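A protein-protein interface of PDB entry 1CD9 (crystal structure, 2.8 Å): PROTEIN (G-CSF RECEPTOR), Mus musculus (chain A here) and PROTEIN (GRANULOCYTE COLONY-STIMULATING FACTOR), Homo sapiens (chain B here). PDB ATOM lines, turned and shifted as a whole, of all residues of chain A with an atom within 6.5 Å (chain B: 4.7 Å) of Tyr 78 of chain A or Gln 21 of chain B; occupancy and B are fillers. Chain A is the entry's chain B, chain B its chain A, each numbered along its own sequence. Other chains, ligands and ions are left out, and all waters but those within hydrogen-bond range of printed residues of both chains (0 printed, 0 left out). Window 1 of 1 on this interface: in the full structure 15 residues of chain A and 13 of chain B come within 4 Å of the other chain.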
ATOM      1  N   LEU A  76     -23.821  20.892  19.956  1.00  0.00           N
ATOM      2  CA  LEU A  76     -23.608  19.789  19.034  1.00  0.00           C
ATOM      3  C   LEU A  76     -24.425  20.243  17.849  1.00  0.00           C
ATOM      4  O   LEU A  76     -25.654  20.157  17.838  1.00  0.00           O
ATOM      5  CB  LEU A  76     -24.149  18.451  19.547  1.00  0.00           C
ATOM      6  CG  LEU A  76     -24.300  17.356  18.476  1.00  0.00           C
ATOM      7  CD1 LEU A  76     -22.977  17.021  17.829  1.00  0.00           C
ATOM      8  CD2 LEU A  76     -24.911  16.123  19.083  1.00  0.00           C
ATOM      9  N   LEU A  77     -23.734  20.830  16.897  1.00  0.00           N
ATOM     10  CA  LEU A  77     -24.378  21.318  15.706  1.00  0.00           C
ATOM     11  C   LEU A  77     -24.932  20.152  14.901  1.00  0.00           C
ATOM     12  O   LEU A  77     -24.361  19.071  14.886  1.00  0.00           O
ATOM     13  CB  LEU A  77     -23.384  22.145  14.889  1.00  0.00           C
ATOM     14  CG  LEU A  77     -22.719  23.307  15.648  1.00  0.00           C
ATOM     15  CD1 LEU A  77     -21.806  24.013  14.734  1.00  0.00           C
ATOM     16  CD2 LEU A  77     -23.718  24.301  16.184  1.00  0.00           C
ATOM     17  N   TYR A  78     -26.054  20.409  14.243  1.00  0.00           N
ATOM     18  CA  TYR A  78     -26.780  19.452  13.432  1.00  0.00           C
ATOM     19  C   TYR A  78     -27.523  18.329  14.136  1.00  0.00           C
ATOM     20  O   TYR A  78     -27.737  17.251  13.585  1.00  0.00           O
ATOM     21  CB  TYR A  78     -25.951  18.952  12.277  1.00  0.00           C
ATOM     22  CG  TYR A  78     -25.416  20.075  11.440  1.00  0.00           C
ATOM     23  CD1 TYR A  78     -26.142  20.638  10.451  1.00  0.00           C
ATOM     24  CD2 TYR A  78     -24.167  20.551  11.624  1.00  0.00           C
ATOM     25  CE1 TYR A  78     -25.616  21.663   9.660  1.00  0.00           C
ATOM     26  CE2 TYR A  78     -23.645  21.564  10.835  1.00  0.00           C
ATOM     27  CZ  TYR A  78     -24.363  22.110   9.865  1.00  0.00           C
ATOM     28  OH  TYR A  78     -23.804  23.074   9.086  1.00  0.00           O
ATOM     29  N   GLN A  79     -27.999  18.642  15.335  1.00  0.00           N
ATOM     30  CA  GLN A  79     -28.813  17.741  16.151  1.00  0.00           C
ATOM     31  C   GLN A  79     -29.666  18.702  16.976  1.00  0.00           C
ATOM     32  O   GLN A  79     -29.236  19.826  17.245  1.00  0.00           O
ATOM     33  CB  GLN A  79     -27.967  16.837  17.061  1.00  0.00           C
ATOM     34  CG  GLN A  79     -28.765  15.679  17.685  1.00  0.00           C
ATOM     35  CD  GLN A  79     -29.772  15.061  16.711  1.00  0.00           C
ATOM     36  OE1 GLN A  79     -29.451  14.146  15.961  1.00  0.00           O
ATOM     37  NE2 GLN A  79     -31.000  15.553  16.734  1.00  0.00           N
ATOM     38  N   TYR A  80     -30.910  18.315  17.253  1.00  0.00           N
ATOM     39  CA  TYR A  80     -31.829  19.145  18.026  1.00  0.00           C
ATOM     40  C   TYR A  80     -31.442  19.245  19.500  1.00  0.00           C
ATOM     41  O   TYR A  80     -30.697  18.419  20.003  1.00  0.00           O
ATOM     42  CB  TYR A  80     -33.256  18.614  17.900  1.00  0.00           C
ATOM     43  CG  TYR A  80     -33.815  18.669  16.500  1.00  0.00           C
ATOM     44  CD1 TYR A  80     -33.328  17.903  15.512  1.00  0.00           C
ATOM     45  CD2 TYR A  80     -34.789  19.528  16.161  1.00  0.00           C
ATOM     46  CE1 TYR A  80     -33.795  18.000  14.201  1.00  0.00           C
ATOM     47  CE2 TYR A  80     -35.262  19.626  14.854  1.00  0.00           C
ATOM     48  CZ  TYR A  80     -34.759  18.866  13.877  1.00  0.00           C
ATOM     49  OH  TYR A  80     -35.196  18.997  12.571  1.00  0.00           O
ATOM     50  N   ASP A 102     -32.147  23.121  16.311  1.00  0.00           N
ATOM     51  CA  ASP A 102     -30.842  22.627  15.933  1.00  0.00           C
ATOM     52  C   ASP A 102     -30.201  23.995  15.730  1.00  0.00           C
ATOM     53  O   ASP A 102     -30.695  24.792  14.950  1.00  0.00           O
ATOM     54  CB  ASP A 102     -30.992  21.893  14.610  1.00  0.00           C
ATOM     55  CG  ASP A 102     -29.690  21.610  13.924  1.00  0.00           C
ATOM     56  OD1 ASP A 102     -28.631  22.137  14.311  1.00  0.00           O
ATOM     57  OD2 ASP A 102     -29.740  20.847  12.952  1.00  0.00           O
ATOM     58  N   PRO A 103     -29.115  24.300  16.451  1.00  0.00           N
ATOM     59  CA  PRO A 103     -28.455  25.602  16.314  1.00  0.00           C
ATOM     60  C   PRO A 103     -28.321  26.067  14.874  1.00  0.00           C
ATOM     61  O   PRO A 103     -28.570  27.217  14.569  1.00  0.00           O
ATOM     62  CB  PRO A 103     -27.087  25.354  16.944  1.00  0.00           C
ATOM     63  CG  PRO A 103     -27.377  24.384  17.972  1.00  0.00           C
ATOM     64  CD  PRO A 103     -28.327  23.412  17.318  1.00  0.00           C
ATOM     65  N   MET A 104     -27.985  25.150  13.983  1.00  0.00           N
ATOM     66  CA  MET A 104     -27.811  25.490  12.587  1.00  0.00           C
ATOM     67  C   MET A 104     -29.078  25.863  11.821  1.00  0.00           C
ATOM     68  O   MET A 104     -28.992  26.344  10.695  1.00  0.00           O
ATOM     69  CB  MET A 104     -27.060  24.374  11.875  1.00  0.00           C
ATOM     70  CG  MET A 104     -25.662  24.202  12.415  1.00  0.00           C
ATOM     71  SD  MET A 104     -24.802  25.788  12.517  1.00  0.00           S
ATOM     72  CE  MET A 104     -24.209  25.901  10.941  1.00  0.00           C
ATOM     73  N   TYR A 143     -20.143  28.214   3.446  1.00  0.00           N
ATOM     74  CA  TYR A 143     -20.296  26.757   3.402  1.00  0.00           C
ATOM     75  C   TYR A 143     -21.736  26.301   3.293  1.00  0.00           C
ATOM     76  O   TYR A 143     -22.027  25.107   3.134  1.00  0.00           O
ATOM     77  CB  TYR A 143     -19.665  26.098   4.625  1.00  0.00           C
ATOM     78  CG  TYR A 143     -20.391  26.382   5.906  1.00  0.00           C
ATOM     79  CD1 TYR A 143     -20.041  27.471   6.690  1.00  0.00           C
ATOM     80  CD2 TYR A 143     -21.491  25.621   6.282  1.00  0.00           C
ATOM     81  CE1 TYR A 143     -20.768  27.801   7.798  1.00  0.00           C
ATOM     82  CE2 TYR A 143     -22.231  25.947   7.387  1.00  0.00           C
ATOM     83  CZ  TYR A 143     -21.861  27.041   8.135  1.00  0.00           C
ATOM     84  OH  TYR A 143     -22.607  27.398   9.208  1.00  0.00           O
ATOM     85  N   MET A 144     -22.631  27.262   3.399  1.00  0.00           N
ATOM     86  CA  MET A 144     -24.054  27.026   3.351  1.00  0.00           C
ATOM     87  C   MET A 144     -24.555  27.261   1.913  1.00  0.00           C
ATOM     88  O   MET A 144     -24.158  28.238   1.281  1.00  0.00           O
ATOM     89  CB  MET A 144     -24.658  28.007   4.334  1.00  0.00           C
ATOM     90  CG  MET A 144     -26.111  27.903   4.534  1.00  0.00           C
ATOM     91  SD  MET A 144     -26.596  29.054   5.810  1.00  0.00           S
ATOM     92  CE  MET A 144     -25.274  28.738   7.042  1.00  0.00           C
ATOM     93  N   ARG A 193     -30.913  30.304   3.429  1.00  0.00           N
ATOM     94  CA  ARG A 193     -30.387  28.949   3.388  1.00  0.00           C
ATOM     95  C   ARG A 193     -31.243  28.138   2.461  1.00  0.00           C
ATOM     96  O   ARG A 193     -32.457  28.152   2.573  1.00  0.00           O
ATOM     97  CB  ARG A 193     -30.416  28.334   4.773  1.00  0.00           C
ATOM     98  CG  ARG A 193     -29.578  27.102   4.915  1.00  0.00           C
ATOM     99  CD  ARG A 193     -29.777  26.598   6.295  1.00  0.00           C
ATOM    100  NE  ARG A 193     -28.940  25.465   6.656  1.00  0.00           N
ATOM    101  CZ  ARG A 193     -29.190  24.670   7.692  1.00  0.00           C
ATOM    102  NH1 ARG A 193     -30.261  24.874   8.448  1.00  0.00           N
ATOM    103  NH2 ARG A 193     -28.326  23.723   8.024  1.00  0.00           N
ATOM    104  N   LEU A 196     -33.224  24.121   3.667  1.00  0.00           N
ATOM    105  CA  LEU A 196     -33.260  23.807   5.069  1.00  0.00           C
ATOM    106  C   LEU A 196     -33.769  25.024   5.806  1.00  0.00           C
ATOM    107  O   LEU A 196     -33.970  26.081   5.235  1.00  0.00           O
ATOM    108  CB  LEU A 196     -31.868  23.416   5.554  1.00  0.00           C
ATOM    109  CG  LEU A 196     -31.269  22.070   5.162  1.00  0.00           C
ATOM    110  CD1 LEU A 196     -29.788  22.072   5.399  1.00  0.00           C
ATOM    111  CD2 LEU A 196     -31.912  20.991   5.966  1.00  0.00           C
ATOM    112  N   LYS B  17     -28.024  18.207   5.569  1.00  0.00           N
ATOM    113  CA  LYS B  17     -27.195  18.683   6.670  1.00  0.00           C
ATOM    114  C   LYS B  17     -25.843  18.003   6.563  1.00  0.00           C
ATOM    115  O   LYS B  17     -24.828  18.621   6.805  1.00  0.00           O
ATOM    116  CB  LYS B  17     -27.810  18.332   8.010  1.00  0.00           C
ATOM    117  CG  LYS B  17     -29.104  19.042   8.290  1.00  0.00           C
ATOM    118  CD  LYS B  17     -29.594  18.744   9.687  1.00  0.00           C
ATOM    119  CE  LYS B  17     -30.817  19.573  10.075  1.00  0.00           C
ATOM    120  NZ  LYS B  17     -31.437  19.169  11.383  1.00  0.00           N
ATOM    121  N   CYS B  18     -25.815  16.725   6.187  1.00  0.00           N
ATOM    122  CA  CYS B  18     -24.539  16.019   6.023  1.00  0.00           C
ATOM    123  C   CYS B  18     -23.707  16.719   4.953  1.00  0.00           C
ATOM    124  O   CYS B  18     -22.537  17.010   5.159  1.00  0.00           O
ATOM    125  CB  CYS B  18     -24.732  14.550   5.648  1.00  0.00           C
ATOM    126  SG  CYS B  18     -25.233  13.500   6.965  1.00  0.00           S
ATOM    127  N   LEU B  19     -24.335  17.070   3.842  1.00  0.00           N
ATOM    128  CA  LEU B  19     -23.631  17.747   2.756  1.00  0.00           C
ATOM    129  C   LEU B  19     -23.107  19.110   3.169  1.00  0.00           C
ATOM    130  O   LEU B  19     -22.118  19.606   2.635  1.00  0.00           O
ATOM    131  CB  LEU B  19     -24.543  17.909   1.560  1.00  0.00           C
ATOM    132  CG  LEU B  19     -24.894  16.646   0.807  1.00  0.00           C
ATOM    133  CD1 LEU B  19     -25.991  16.965  -0.125  1.00  0.00           C
ATOM    134  CD2 LEU B  19     -23.698  16.128   0.058  1.00  0.00           C
ATOM    135  N   GLU B  20     -23.778  19.729   4.117  1.00  0.00           N
ATOM    136  CA  GLU B  20     -23.348  21.031   4.573  1.00  0.00           C
ATOM    137  C   GLU B  20     -22.191  20.874   5.540  1.00  0.00           C
ATOM    138  O   GLU B  20     -21.306  21.715   5.598  1.00  0.00           O
ATOM    139  CB  GLU B  20     -24.517  21.735   5.227  1.00  0.00           C
ATOM    140  CG  GLU B  20     -24.227  23.120   5.593  1.00  0.00           C
ATOM    141  CD  GLU B  20     -25.450  23.809   6.100  1.00  0.00           C
ATOM    142  OE1 GLU B  20     -26.323  24.160   5.329  1.00  0.00           O
ATOM    143  OE2 GLU B  20     -25.589  24.002   7.292  1.00  0.00           O
ATOM    144  N   GLN B  21     -22.211  19.799   6.321  1.00  0.00           N
ATOM    145  CA  GLN B  21     -21.141  19.545   7.255  1.00  0.00           C
ATOM    146  C   GLN B  21     -19.914  19.188   6.445  1.00  0.00           C
ATOM    147  O   GLN B  21     -18.823  19.652   6.738  1.00  0.00           O
ATOM    148  CB  GLN B  21     -21.520  18.436   8.205  1.00  0.00           C
ATOM    149  CG  GLN B  21     -22.491  18.892   9.242  1.00  0.00           C
ATOM    150  CD  GLN B  21     -22.676  17.920  10.383  1.00  0.00           C
ATOM    151  OE1 GLN B  21     -23.564  17.062  10.345  1.00  0.00           O
ATOM    152  NE2 GLN B  21     -21.866  18.066  11.425  1.00  0.00           N
ATOM    153  N   VAL B  22     -20.099  18.438   5.369  1.00  0.00           N
ATOM    154  CA  VAL B  22     -18.960  18.105   4.541  1.00  0.00           C
ATOM    155  C   VAL B  22     -18.316  19.378   4.018  1.00  0.00           C
ATOM    156  O   VAL B  22     -17.113  19.539   4.090  1.00  0.00           O
ATOM    157  CB  VAL B  22     -19.308  17.169   3.389  1.00  0.00           C
ATOM    158  CG1 VAL B  22     -18.226  17.190   2.361  1.00  0.00           C
ATOM    159  CG2 VAL B  22     -19.469  15.763   3.922  1.00  0.00           C
ATOM    160  N   ARG B  23     -19.098  20.317   3.525  1.00  0.00           N
ATOM    161  CA  ARG B  23     -18.500  21.547   3.020  1.00  0.00           C
ATOM    162  C   ARG B  23     -17.831  22.387   4.076  1.00  0.00           C
ATOM    163  O   ARG B  23     -16.816  23.021   3.800  1.00  0.00           O
ATOM    164  CB  ARG B  23     -19.523  22.435   2.366  1.00  0.00           C
ATOM    165  CG  ARG B  23     -19.906  22.036   1.000  1.00  0.00           C
ATOM    166  CD  ARG B  23     -20.981  22.981   0.515  1.00  0.00           C
ATOM    167  NE  ARG B  23     -21.999  22.182  -0.141  1.00  0.00           N
ATOM    168  CZ  ARG B  23     -23.267  22.149   0.226  1.00  0.00           C
ATOM    169  NH1 ARG B  23     -23.683  22.899   1.240  1.00  0.00           N
ATOM    170  NH2 ARG B  23     -24.089  21.310  -0.386  1.00  0.00           N
ATOM    171  N   LYS B  24     -18.437  22.457   5.256  1.00  0.00           N
ATOM    172  CA  LYS B  24     -17.908  23.238   6.365  1.00  0.00           C
ATOM    173  C   LYS B  24     -16.528  22.703   6.741  1.00  0.00           C
ATOM    174  O   LYS B  24     -15.553  23.462   6.804  1.00  0.00           O
ATOM    175  CB  LYS B  24     -18.891  23.156   7.534  1.00  0.00           C
ATOM    176  CG  LYS B  24     -18.552  23.962   8.747  1.00  0.00           C
ATOM    177  CD  LYS B  24     -19.606  23.738   9.820  1.00  0.00           C
ATOM    178  CE  LYS B  24     -19.349  24.585  11.066  1.00  0.00           C
ATOM    179  NZ  LYS B  24     -19.115  26.035  10.768  1.00  0.00           N
ATOM    180  N   ILE B  25     -16.438  21.386   6.919  1.00  0.00           N
ATOM    181  CA  ILE B  25     -15.185  20.731   7.253  1.00  0.00           C
ATOM    182  C   ILE B  25     -14.190  20.892   6.108  1.00  0.00           C
ATOM    183  O   ILE B  25     -13.023  21.088   6.340  1.00  0.00           O
ATOM    184  CB  ILE B  25     -15.407  19.256   7.541  1.00  0.00           C
ATOM    185  CG1 ILE B  25     -16.252  19.112   8.791  1.00  0.00           C
ATOM    186  CG2 ILE B  25     -14.095  18.539   7.723  1.00  0.00           C
ATOM    187  CD1 ILE B  25     -16.840  17.749   8.966  1.00  0.00           C
ATOM    188  N   ASP B 110     -15.430  20.243  14.423  1.00  0.00           N
ATOM    189  CA  ASP B 110     -16.329  20.050  13.300  1.00  0.00           C
ATOM    190  C   ASP B 110     -16.371  18.616  12.822  1.00  0.00           C
ATOM    191  O   ASP B 110     -17.454  18.124  12.503  1.00  0.00           O
ATOM    192  CB  ASP B 110     -16.006  21.019  12.169  1.00  0.00           C
ATOM    193  CG  ASP B 110     -16.498  22.422  12.465  1.00  0.00           C
ATOM    194  OD1 ASP B 110     -17.720  22.592  12.631  1.00  0.00           O
ATOM    195  OD2 ASP B 110     -15.683  23.354  12.556  1.00  0.00           O
ATOM    196  N   ASP B 113     -18.267  16.337  15.656  1.00  0.00           N
ATOM    197  CA  ASP B 113     -19.723  16.467  15.612  1.00  0.00           C
ATOM    198  C   ASP B 113     -20.331  15.860  14.376  1.00  0.00           C
ATOM    199  O   ASP B 113     -21.410  15.327  14.429  1.00  0.00           O
ATOM    200  CB  ASP B 113     -20.130  17.919  15.696  1.00  0.00           C
ATOM    201  CG  ASP B 113     -19.739  18.560  17.014  1.00  0.00           C
ATOM    202  OD1 ASP B 113     -18.861  18.034  17.737  1.00  0.00           O
ATOM    203  OD2 ASP B 113     -20.326  19.609  17.326  1.00  0.00           O
ATOM    204  N   PHE B 114     -19.654  15.951  13.248  1.00  0.00           N
ATOM    205  CA  PHE B 114     -20.200  15.351  12.061  1.00  0.00           C
ATOM    206  C   PHE B 114     -20.245  13.862  12.306  1.00  0.00           C
ATOM    207  O   PHE B 114     -21.199  13.197  11.945  1.00  0.00           O
ATOM    208  CB  PHE B 114     -19.308  15.654  10.879  1.00  0.00           C
ATOM    209  CG  PHE B 114     -19.850  15.177   9.569  1.00  0.00           C
ATOM    210  CD1 PHE B 114     -21.151  14.744   9.454  1.00  0.00           C
ATOM    211  CD2 PHE B 114     -19.043  15.144   8.442  1.00  0.00           C
ATOM    212  CE1 PHE B 114     -21.647  14.285   8.250  1.00  0.00           C
ATOM    213  CE2 PHE B 114     -19.544  14.679   7.216  1.00  0.00           C
ATOM    214  CZ  PHE B 114     -20.850  14.250   7.133  1.00  0.00           C
ATOM    215  N   THR B 117     -23.138  13.197  14.796  1.00  0.00           N
ATOM    216  CA  THR B 117     -24.364  13.438  14.085  1.00  0.00           C
ATOM    217  C   THR B 117     -24.777  12.214  13.299  1.00  0.00           C
ATOM    218  O   THR B 117     -25.926  11.793  13.338  1.00  0.00           O
ATOM    219  CB  THR B 117     -24.082  14.613  13.178  1.00  0.00           C
ATOM    220  OG1 THR B 117     -24.329  15.804  13.919  1.00  0.00           O
ATOM    221  CG2 THR B 117     -24.844  14.565  11.879  1.00  0.00           C
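The side-chain amino group (NZ) of Lys 17 of chain B is in salt-bridge range of the side-chain carboxylate (OD2) of Asp 102 of chain A (2.9 Å). OE2 of Glu 20 of chain B is in hydrogen-bond range of OH of Tyr 78 of chain A (2.7 Å). The side-chain hydroxyl (OG1) of Thr 117 of chain B sits at hydrogen-bond distance from the backbone carbonyl oxygen (O) of Leu 77 of chain A (3.4 Å). The backbone carbonyl oxygen (O) of Tyr 143 of chain A lies within hydrogen-bond range of the guanidinium group (NH1) of Arg 23 of chain B (3.3 Å). The side-chain carboxylate (OE2) of Glu 20 of chain B is in salt-bridge range of the guanidinium group (NH2) of Arg 193 of chain A, at 2.8 Å.
O of Asp 113 of chain B lies within hydrogen-bond range of OG1 of Thr 117 of chain B (3.0 Å). The backbone NH (N) of Met 104 of chain A lies close to the side-chain carboxylate (OD1) of Asp 102 of chain A (3.1 Å). The backbone carbonyl oxygen of Met 104 of chain A lies within hydrogen-bond range of the guanidinium group of Arg 193 of chain A, at 3.0 Å. N of Tyr 78 of chain A is in hydrogen-bond range of OD1 of Asp 102 of chain A (3.1 Å).
Among the printed residues, pairs that only touch across the chains: Leu 76 of chain A with Asp 113 of chain B (3.7 Å), Leu 77 of chain A with Asp 113 of chain B (3.6 Å), Tyr 78 of chain A with Lys 17 of chain B (3.7 Å), Tyr 78 of chain A with Gln 21 of chain B (3.3 Å), Tyr 78 of chain A with Thr 117 of chain B (3.7 Å), Tyr 80 of chain A with Lys 17 of chain B (3.9 Å), Tyr 143 of chain A with Glu 20 of chain B (3.8 Å), Tyr 143 of chain A with Lys 24 of chain B (3.8 Å) and Met 144 of chain A with Glu 20 of chain B (3.8 Å).
Of the printed residues of chain B, Leu 77 of chain A touches Asp 113 (3.6 Å) and Thr 117 (3.4 Å). Of chain B, only Lys 17, Glu 20, Gln 21 and Thr 117 come within 4 Å of Tyr 78 of chain A. Gln 21 of chain B touches just one residue of chain A: Tyr 78. Of the printed residues of chain A, Arg 23 of chain B touches Tyr 143. The nearest residue of chain A that does not touch Gln 21 of chain B is Leu 77 of chain A (4.4 Å). The nearest printed residue of chain B that does not touch Met 144 of chain A is Arg 23 of chain B (4.5 Å).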
